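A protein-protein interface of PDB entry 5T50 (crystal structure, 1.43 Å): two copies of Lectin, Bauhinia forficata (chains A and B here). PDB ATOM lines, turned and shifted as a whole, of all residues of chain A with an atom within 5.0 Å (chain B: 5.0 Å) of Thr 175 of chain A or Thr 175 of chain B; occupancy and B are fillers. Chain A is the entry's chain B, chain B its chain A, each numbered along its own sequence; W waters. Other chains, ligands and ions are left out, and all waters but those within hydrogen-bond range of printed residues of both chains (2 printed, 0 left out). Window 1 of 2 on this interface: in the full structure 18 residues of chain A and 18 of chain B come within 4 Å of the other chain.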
ATOM      1  N   HIS A 164     -15.132 -22.593  13.511  1.00  0.00           N
ATOM      2  CA  HIS A 164     -16.393 -21.909  13.260  1.00  0.00           C
ATOM      3  C   HIS A 164     -16.464 -20.770  14.269  1.00  0.00           C
ATOM      4  O   HIS A 164     -16.365 -21.044  15.469  1.00  0.00           O
ATOM      5  CB  HIS A 164     -17.609 -22.810  13.501  1.00  0.00           C
ATOM      6  CG  HIS A 164     -17.602 -24.092  12.720  1.00  0.00           C
ATOM      7  ND1 HIS A 164     -18.132 -24.208  11.449  1.00  0.00           N
ATOM      8  CD2 HIS A 164     -17.045 -25.290  12.993  1.00  0.00           C
ATOM      9  CE1 HIS A 164     -17.932 -25.442  11.009  1.00  0.00           C
ATOM     10  NE2 HIS A 164     -17.317 -26.122  11.943  1.00  0.00           N
ATOM     11  N   VAL A 165     -16.605 -19.528  13.816  1.00  0.00           N
ATOM     12  CA  VAL A 165     -16.711 -18.427  14.727  1.00  0.00           C
ATOM     13  C   VAL A 165     -17.945 -17.611  14.382  1.00  0.00           C
ATOM     14  O   VAL A 165     -18.175 -17.261  13.224  1.00  0.00           O
ATOM     15  CB  VAL A 165     -15.435 -17.534  14.694  1.00  0.00           C
ATOM     16  CG1 VAL A 165     -15.571 -16.355  15.629  1.00  0.00           C
ATOM     17  CG2 VAL A 165     -14.200 -18.346  15.009  1.00  0.00           C
ATOM     18  N   GLY A 166     -18.825 -17.436  15.376  1.00  0.00           N
ATOM     19  CA  GLY A 166     -20.027 -16.680  15.145  1.00  0.00           C
ATOM     20  C   GLY A 166     -20.289 -15.609  16.169  1.00  0.00           C
ATOM     21  O   GLY A 166     -19.828 -15.705  17.321  1.00  0.00           O
ATOM     22  N   ILE A 173     -23.033 -12.245  21.845  1.00  0.00           N
ATOM     23  CA  ILE A 173     -22.223 -13.379  22.233  1.00  0.00           C
ATOM     24  C   ILE A 173     -21.366 -13.821  21.056  1.00  0.00           C
ATOM     25  O   ILE A 173     -21.871 -14.047  19.929  1.00  0.00           O
ATOM     26  CB  ILE A 173     -23.101 -14.572  22.690  1.00  0.00           C
ATOM     27  CG1 ILE A 173     -23.711 -14.232  24.051  1.00  0.00           C
ATOM     28  CG2 ILE A 173     -22.214 -15.817  22.823  1.00  0.00           C
ATOM     29  CD1 ILE A 173     -24.839 -15.199  24.497  1.00  0.00           C
ATOM     30  N   LEU A 174     -20.067 -13.923  21.374  1.00  0.00           N
ATOM     31  CA  LEU A 174     -19.076 -14.447  20.409  1.00  0.00           C
ATOM     32  C   LEU A 174     -18.740 -15.882  20.774  1.00  0.00           C
ATOM     33  O   LEU A 174     -18.420 -16.169  21.945  1.00  0.00           O
ATOM     34  CB  LEU A 174     -17.785 -13.599  20.483  1.00  0.00           C
ATOM     35  CG  LEU A 174     -16.657 -14.001  19.499  1.00  0.00           C
ATOM     36  CD1 LEU A 174     -17.042 -13.695  18.071  1.00  0.00           C
ATOM     37  CD2 LEU A 174     -15.350 -13.235  19.846  1.00  0.00           C
ATOM     38  N   THR A 175     -18.807 -16.802  19.811  1.00  0.00           N
ATOM     39  CA  THR A 175     -18.573 -18.207  20.055  1.00  0.00           C
ATOM     40  C   THR A 175     -17.587 -18.760  19.021  1.00  0.00           C
ATOM     41  O   THR A 175     -17.717 -18.478  17.791  1.00  0.00           O
ATOM     42  CB  THR A 175     -19.926 -19.019  19.908  1.00  0.00           C
ATOM     43  OG1 THR A 175     -20.785 -18.562  20.929  1.00  0.00           O
ATOM     44  CG2 THR A 175     -19.717 -20.472  20.031  1.00  0.00           C
ATOM     45  N   ALA A 176     -16.737 -19.663  19.499  1.00  0.00           N
ATOM     46  CA  ALA A 176     -15.901 -20.446  18.613  1.00  0.00           C
ATOM     47  C   ALA A 176     -16.122 -21.937  18.855  1.00  0.00           C
ATOM     48  O   ALA A 176     -16.100 -22.387  20.023  1.00  0.00           O
ATOM     49  CB  ALA A 176     -14.405 -20.108  18.834  1.00  0.00           C
ATOM     50  N   PHE A 177     -16.298 -22.696  17.786  1.00  0.00           N
ATOM     51  CA  PHE A 177     -16.223 -24.133  17.830  1.00  0.00           C
ATOM     52  C   PHE A 177     -15.003 -24.557  16.985  1.00  0.00           C
ATOM     53  O   PHE A 177     -14.858 -24.058  15.843  1.00  0.00           O
ATOM     54  CB  PHE A 177     -17.406 -24.843  17.178  1.00  0.00           C
ATOM     55  CG  PHE A 177     -18.783 -24.524  17.791  1.00  0.00           C
ATOM     56  CD1 PHE A 177     -18.958 -24.132  19.113  1.00  0.00           C
ATOM     57  CD2 PHE A 177     -19.893 -24.581  16.982  1.00  0.00           C
ATOM     58  CE1 PHE A 177     -20.231 -23.798  19.583  1.00  0.00           C
ATOM     59  CE2 PHE A 177     -21.154 -24.297  17.479  1.00  0.00           C
ATOM     60  CZ  PHE A 177     -21.306 -23.943  18.761  1.00  0.00           C
ATOM     61  N   LEU A 188     -15.958 -22.435  23.003  1.00  0.00           N
ATOM     62  CA  LEU A 188     -15.750 -21.256  23.804  1.00  0.00           C
ATOM     63  C   LEU A 188     -16.724 -20.165  23.455  1.00  0.00           C
ATOM     64  O   LEU A 188     -16.849 -19.839  22.273  1.00  0.00           O
ATOM     65  CB  LEU A 188     -14.318 -20.637  23.630  1.00  0.00           C
ATOM     66  CG  LEU A 188     -13.139 -21.467  23.934  1.00  0.00           C
ATOM     67  CD1 LEU A 188     -11.963 -20.562  23.833  1.00  0.00           C
ATOM     68  CD2 LEU A 188     -13.217 -21.907  25.362  1.00  0.00           C
ATOM     69  N   SER A 189     -17.411 -19.603  24.449  1.00  0.00           N
ATOM     70  CA  SER A 189     -18.313 -18.533  24.220  1.00  0.00           C
ATOM     71  C   SER A 189     -18.105 -17.401  25.241  1.00  0.00           C
ATOM     72  O   SER A 189     -17.729 -17.662  26.380  1.00  0.00           O
ATOM     73  CB  SER A 189     -19.783 -19.060  24.333  1.00  0.00           C
ATOM     74  OG  SER A 189     -20.166 -19.878  23.265  1.00  0.00           O
ATOM     75  N   HIS B 164     -24.593 -27.096  13.916  1.00  0.00           N
ATOM     76  CA  HIS B 164     -23.609 -27.232  14.943  1.00  0.00           C
ATOM     77  C   HIS B 164     -24.231 -26.664  16.232  1.00  0.00           C
ATOM     78  O   HIS B 164     -24.666 -25.509  16.231  1.00  0.00           O
ATOM     79  CB  HIS B 164     -22.355 -26.421  14.640  1.00  0.00           C
ATOM     80  CG  HIS B 164     -21.764 -26.682  13.308  1.00  0.00           C
ATOM     81  ND1 HIS B 164     -20.811 -27.637  13.130  1.00  0.00           N
ATOM     82  CD2 HIS B 164     -22.032 -26.157  12.098  1.00  0.00           C
ATOM     83  CE1 HIS B 164     -20.471 -27.651  11.843  1.00  0.00           C
ATOM     84  NE2 HIS B 164     -21.198 -26.768  11.194  1.00  0.00           N
ATOM     85  N   VAL B 165     -24.268 -27.457  17.314  1.00  0.00           N
ATOM     86  CA  VAL B 165     -24.845 -26.974  18.603  1.00  0.00           C
ATOM     87  C   VAL B 165     -23.769 -27.220  19.663  1.00  0.00           C
ATOM     88  O   VAL B 165     -23.295 -28.344  19.788  1.00  0.00           O
ATOM     89  CB  VAL B 165     -26.193 -27.639  18.931  1.00  0.00           C
ATOM     90  CG1 VAL B 165     -26.712 -27.200  20.271  1.00  0.00           C
ATOM     91  CG2 VAL B 165     -27.203 -27.421  17.797  1.00  0.00           C
ATOM     92  N   GLY B 166     -23.414 -26.161  20.384  1.00  0.00           N
ATOM     93  CA  GLY B 166     -22.413 -26.261  21.395  1.00  0.00           C
ATOM     94  C   GLY B 166     -22.898 -25.653  22.688  1.00  0.00           C
ATOM     95  O   GLY B 166     -23.704 -24.706  22.688  1.00  0.00           O
ATOM     96  N   ILE B 173     -23.459 -20.936  28.120  1.00  0.00           N
ATOM     97  CA  ILE B 173     -24.010 -20.421  26.853  1.00  0.00           C
ATOM     98  C   ILE B 173     -24.217 -21.543  25.836  1.00  0.00           C
ATOM     99  O   ILE B 173     -23.295 -22.355  25.580  1.00  0.00           O
ATOM    100  CB  ILE B 173     -23.109 -19.354  26.220  1.00  0.00           C
ATOM    101  CG1 ILE B 173     -23.059 -18.116  27.089  1.00  0.00           C
ATOM    102  CG2 ILE B 173     -23.541 -19.020  24.783  1.00  0.00           C
ATOM    103  CD1 ILE B 173     -22.035 -17.046  26.755  1.00  0.00           C
ATOM    104  N   LEU B 174     -25.467 -21.631  25.346  1.00  0.00           N
ATOM    105  CA  LEU B 174     -25.853 -22.563  24.281  1.00  0.00           C
ATOM    106  C   LEU B 174     -25.848 -21.792  22.948  1.00  0.00           C
ATOM    107  O   LEU B 174     -26.485 -20.749  22.842  1.00  0.00           O
ATOM    108  CB  LEU B 174     -27.227 -23.109  24.575  1.00  0.00           C
ATOM    109  CG  LEU B 174     -27.818 -24.127  23.623  1.00  0.00           C
ATOM    110  CD1 LEU B 174     -27.017 -25.420  23.629  1.00  0.00           C
ATOM    111  CD2 LEU B 174     -29.302 -24.348  23.955  1.00  0.00           C
ATOM    112  N   THR B 175     -25.214 -22.381  21.933  1.00  0.00           N
ATOM    113  CA  THR B 175     -25.117 -21.779  20.622  1.00  0.00           C
ATOM    114  C   THR B 175     -25.474 -22.779  19.541  1.00  0.00           C
ATOM    115  O   THR B 175     -25.010 -23.933  19.583  1.00  0.00           O
ATOM    116  CB  THR B 175     -23.680 -21.230  20.395  1.00  0.00           C
ATOM    117  OG1 THR B 175     -23.353 -20.254  21.370  1.00  0.00           O
ATOM    118  CG2 THR B 175     -23.460 -20.694  18.989  1.00  0.00           C
ATOM    119  N   ALA B 176     -26.202 -22.292  18.549  1.00  0.00           N
ATOM    120  CA  ALA B 176     -26.428 -23.025  17.286  1.00  0.00           C
ATOM    121  C   ALA B 176     -25.917 -22.195  16.100  1.00  0.00           C
ATOM    122  O   ALA B 176     -26.206 -20.992  16.002  1.00  0.00           O
ATOM    123  CB  ALA B 176     -27.908 -23.289  17.083  1.00  0.00           C
ATOM    124  N   PHE B 177     -25.178 -22.901  15.240  1.00  0.00           N
ATOM    125  CA  PHE B 177     -24.836 -22.418  13.907  1.00  0.00           C
ATOM    126  C   PHE B 177     -25.488 -23.354  12.902  1.00  0.00           C
ATOM    127  O   PHE B 177     -25.328 -24.590  13.001  1.00  0.00           O
ATOM    128  CB  PHE B 177     -23.332 -22.429  13.624  1.00  0.00           C
ATOM    129  CG  PHE B 177     -22.443 -21.623  14.559  1.00  0.00           C
ATOM    130  CD1 PHE B 177     -22.870 -20.504  15.248  1.00  0.00           C
ATOM    131  CD2 PHE B 177     -21.150 -22.018  14.739  1.00  0.00           C
ATOM    132  CE1 PHE B 177     -22.028 -19.773  16.046  1.00  0.00           C
ATOM    133  CE2 PHE B 177     -20.275 -21.278  15.581  1.00  0.00           C
ATOM    134  CZ  PHE B 177     -20.720 -20.186  16.225  1.00  0.00           C
ATOM    135  N   LEU B 188     -27.388 -18.360  16.594  1.00  0.00           N
ATOM    136  CA  LEU B 188     -28.204 -18.056  17.782  1.00  0.00           C
ATOM    137  C   LEU B 188     -27.464 -18.490  18.998  1.00  0.00           C
ATOM    138  O   LEU B 188     -26.998 -19.641  19.064  1.00  0.00           O
ATOM    139  CB  LEU B 188     -29.563 -18.858  17.797  1.00  0.00           C
ATOM    140  CG  LEU B 188     -30.578 -18.522  16.735  1.00  0.00           C
ATOM    141  CD1 LEU B 188     -31.866 -19.278  17.062  1.00  0.00           C
ATOM    142  CD2 LEU B 188     -30.932 -17.042  16.814  1.00  0.00           C
ATOM    143  N   SER B 189     -27.366 -17.597  19.991  1.00  0.00           N
ATOM    144  CA  SER B 189     -26.685 -17.935  21.264  1.00  0.00           C
ATOM    145  C   SER B 189     -27.591 -17.456  22.415  1.00  0.00           C
ATOM    146  O   SER B 189     -28.211 -16.418  22.302  1.00  0.00           O
ATOM    147  CB  SER B 189     -25.344 -17.219  21.372  1.00  0.00           C
ATOM    148  OG  SER B 189     -24.459 -17.802  20.430  1.00  0.00           O
HETATM  149  O   HOH W   1     -22.333 -16.817  19.199  1.00  0.00           O
HETATM  150  O   HOH W   2     -21.907 -21.923  23.064  1.00  0.00           O
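Water W1 lies within hydrogen-bond range of OG of Ser 189 of chain B (2.6 Å), O of Ile 173 of chain A (2.9 Å), OG1 of Thr 175 of chain A (2.9 Å) and O of Gly 166 of chain A (3.3 Å).
Water W2 lies within hydrogen-bond range of OG of Ser 189 of chain A, OG1 of Thr 175 of chain B, O of Ile 173 of chain B and O of Gly 166 of chain B.
Among the printed residues, pairs that only touch across the chains: His 164 of chain A with His 164 of chain B (3.5 Å), His 164 of chain A with Phe 177 of chain B (3.7 Å), Gly 166 of chain A with Phe 177 of chain B (3.4 Å), Ile 173 of chain A with Ile 173 of chain B (3.98 Å), Ile 173 of chain A with Ser 189 of chain B (3.7 Å), Thr 175 of chain A with Phe 177 of chain B (3.8 Å), Thr 175 of chain A with Ser 189 of chain B (3.8 Å), Phe 177 of chain A with His 164 of chain B (3.7 Å), Phe 177 of chain A with Gly 166 of chain B (3.5 Å), Phe 177 of chain A with Thr 175 of chain B (3.8 Å), Phe 177 of chain A with Phe 177 of chain B (3.6 Å), Ser 189 of chain A with Ile 173 of chain B (3.8 Å) and Ser 189 of chain A with Thr 175 of chain B (3.7 Å).
His 164 of chain B touches its own counterpart, His 164 of chain A.
Ile 173 of chain A touches Ser 189 of chain B, and with the chains exchanged Ser 189 of chain A touches Ile 173 of chain B.
Thr 175 of chain A touches its own counterpart, Thr 175 of chain B.
Phe 177 of chain A touches its own counterpart, Phe 177 of chain B.
10 positions are printed for both chains.
Of the 14 pairs that touch across the chains among the printed residues, 14 have their exchanged pair printed and touching as well.
O of Phe 177 of chain B is in hydrogen-bond range of N of His 164 of chain B, at 2.8 Å.
N of Gly 166 of chain B lies within hydrogen-bond range of O of Thr 175 of chain B (2.9 Å).
The side-chain hydroxyl (OG1) of Thr 175 of chain B sits at hydrogen-bond distance from the side-chain hydroxyl (OG) of Ser 189 of chain B.
The backbone carbonyl oxygen of Phe 177 of chain A lies within hydrogen-bond range of the backbone NH of His 164 of chain A, 2.8 Å away.
N of Gly 166 of chain A sits at hydrogen-bond distance from O of Thr 175 of chain A (2.9 Å).
The side-chain hydroxyl of Thr 175 of chain A sits at hydrogen-bond distance from the side-chain hydroxyl of Ser 189 of chain A (2.8 Å).
Of the printed residues of chain B, His 164 of chain A touches His 164 and Phe 177.
Of chain B, only Thr 175 (3.1 Å), Phe 177 (3.8 Å) and Ser 189 (3.8 Å) come within 4 Å of Thr 175 of chain A.
Val 165 of chain B touches none of the printed residues of chain A.
Of the printed residues of chain A, Gly 166 of chain B touches Phe 177 (3.5 Å).
Printed residues of chain A within 4 Å of Ile 173 of chain B: Ile 173 (3.98 Å) and Ser 189 (3.8 Å).
Thr 175 of chain B touches just these residues of chain A: Thr 175, Phe 177 and Ser 189.
OG1 of Thr 175 of chain A sits at hydrogen-bond distance from OG1 of Thr 175 of chain B, 3.1 Å away.
Hydrophobic or aromatic side chains of chain A within 4 Å of the printed part of chain B: His 164, Ile 173 and Phe 177.
Of the 10 printed residues of chain B, 6 touch a printed residue of chain A.
Among the printed residues, 14 pairs touch across the chains.
Among the printed residues, no Asp or Glu carboxylate lies within 4 Å of a Lys or Arg side-chain nitrogen of the other chain.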
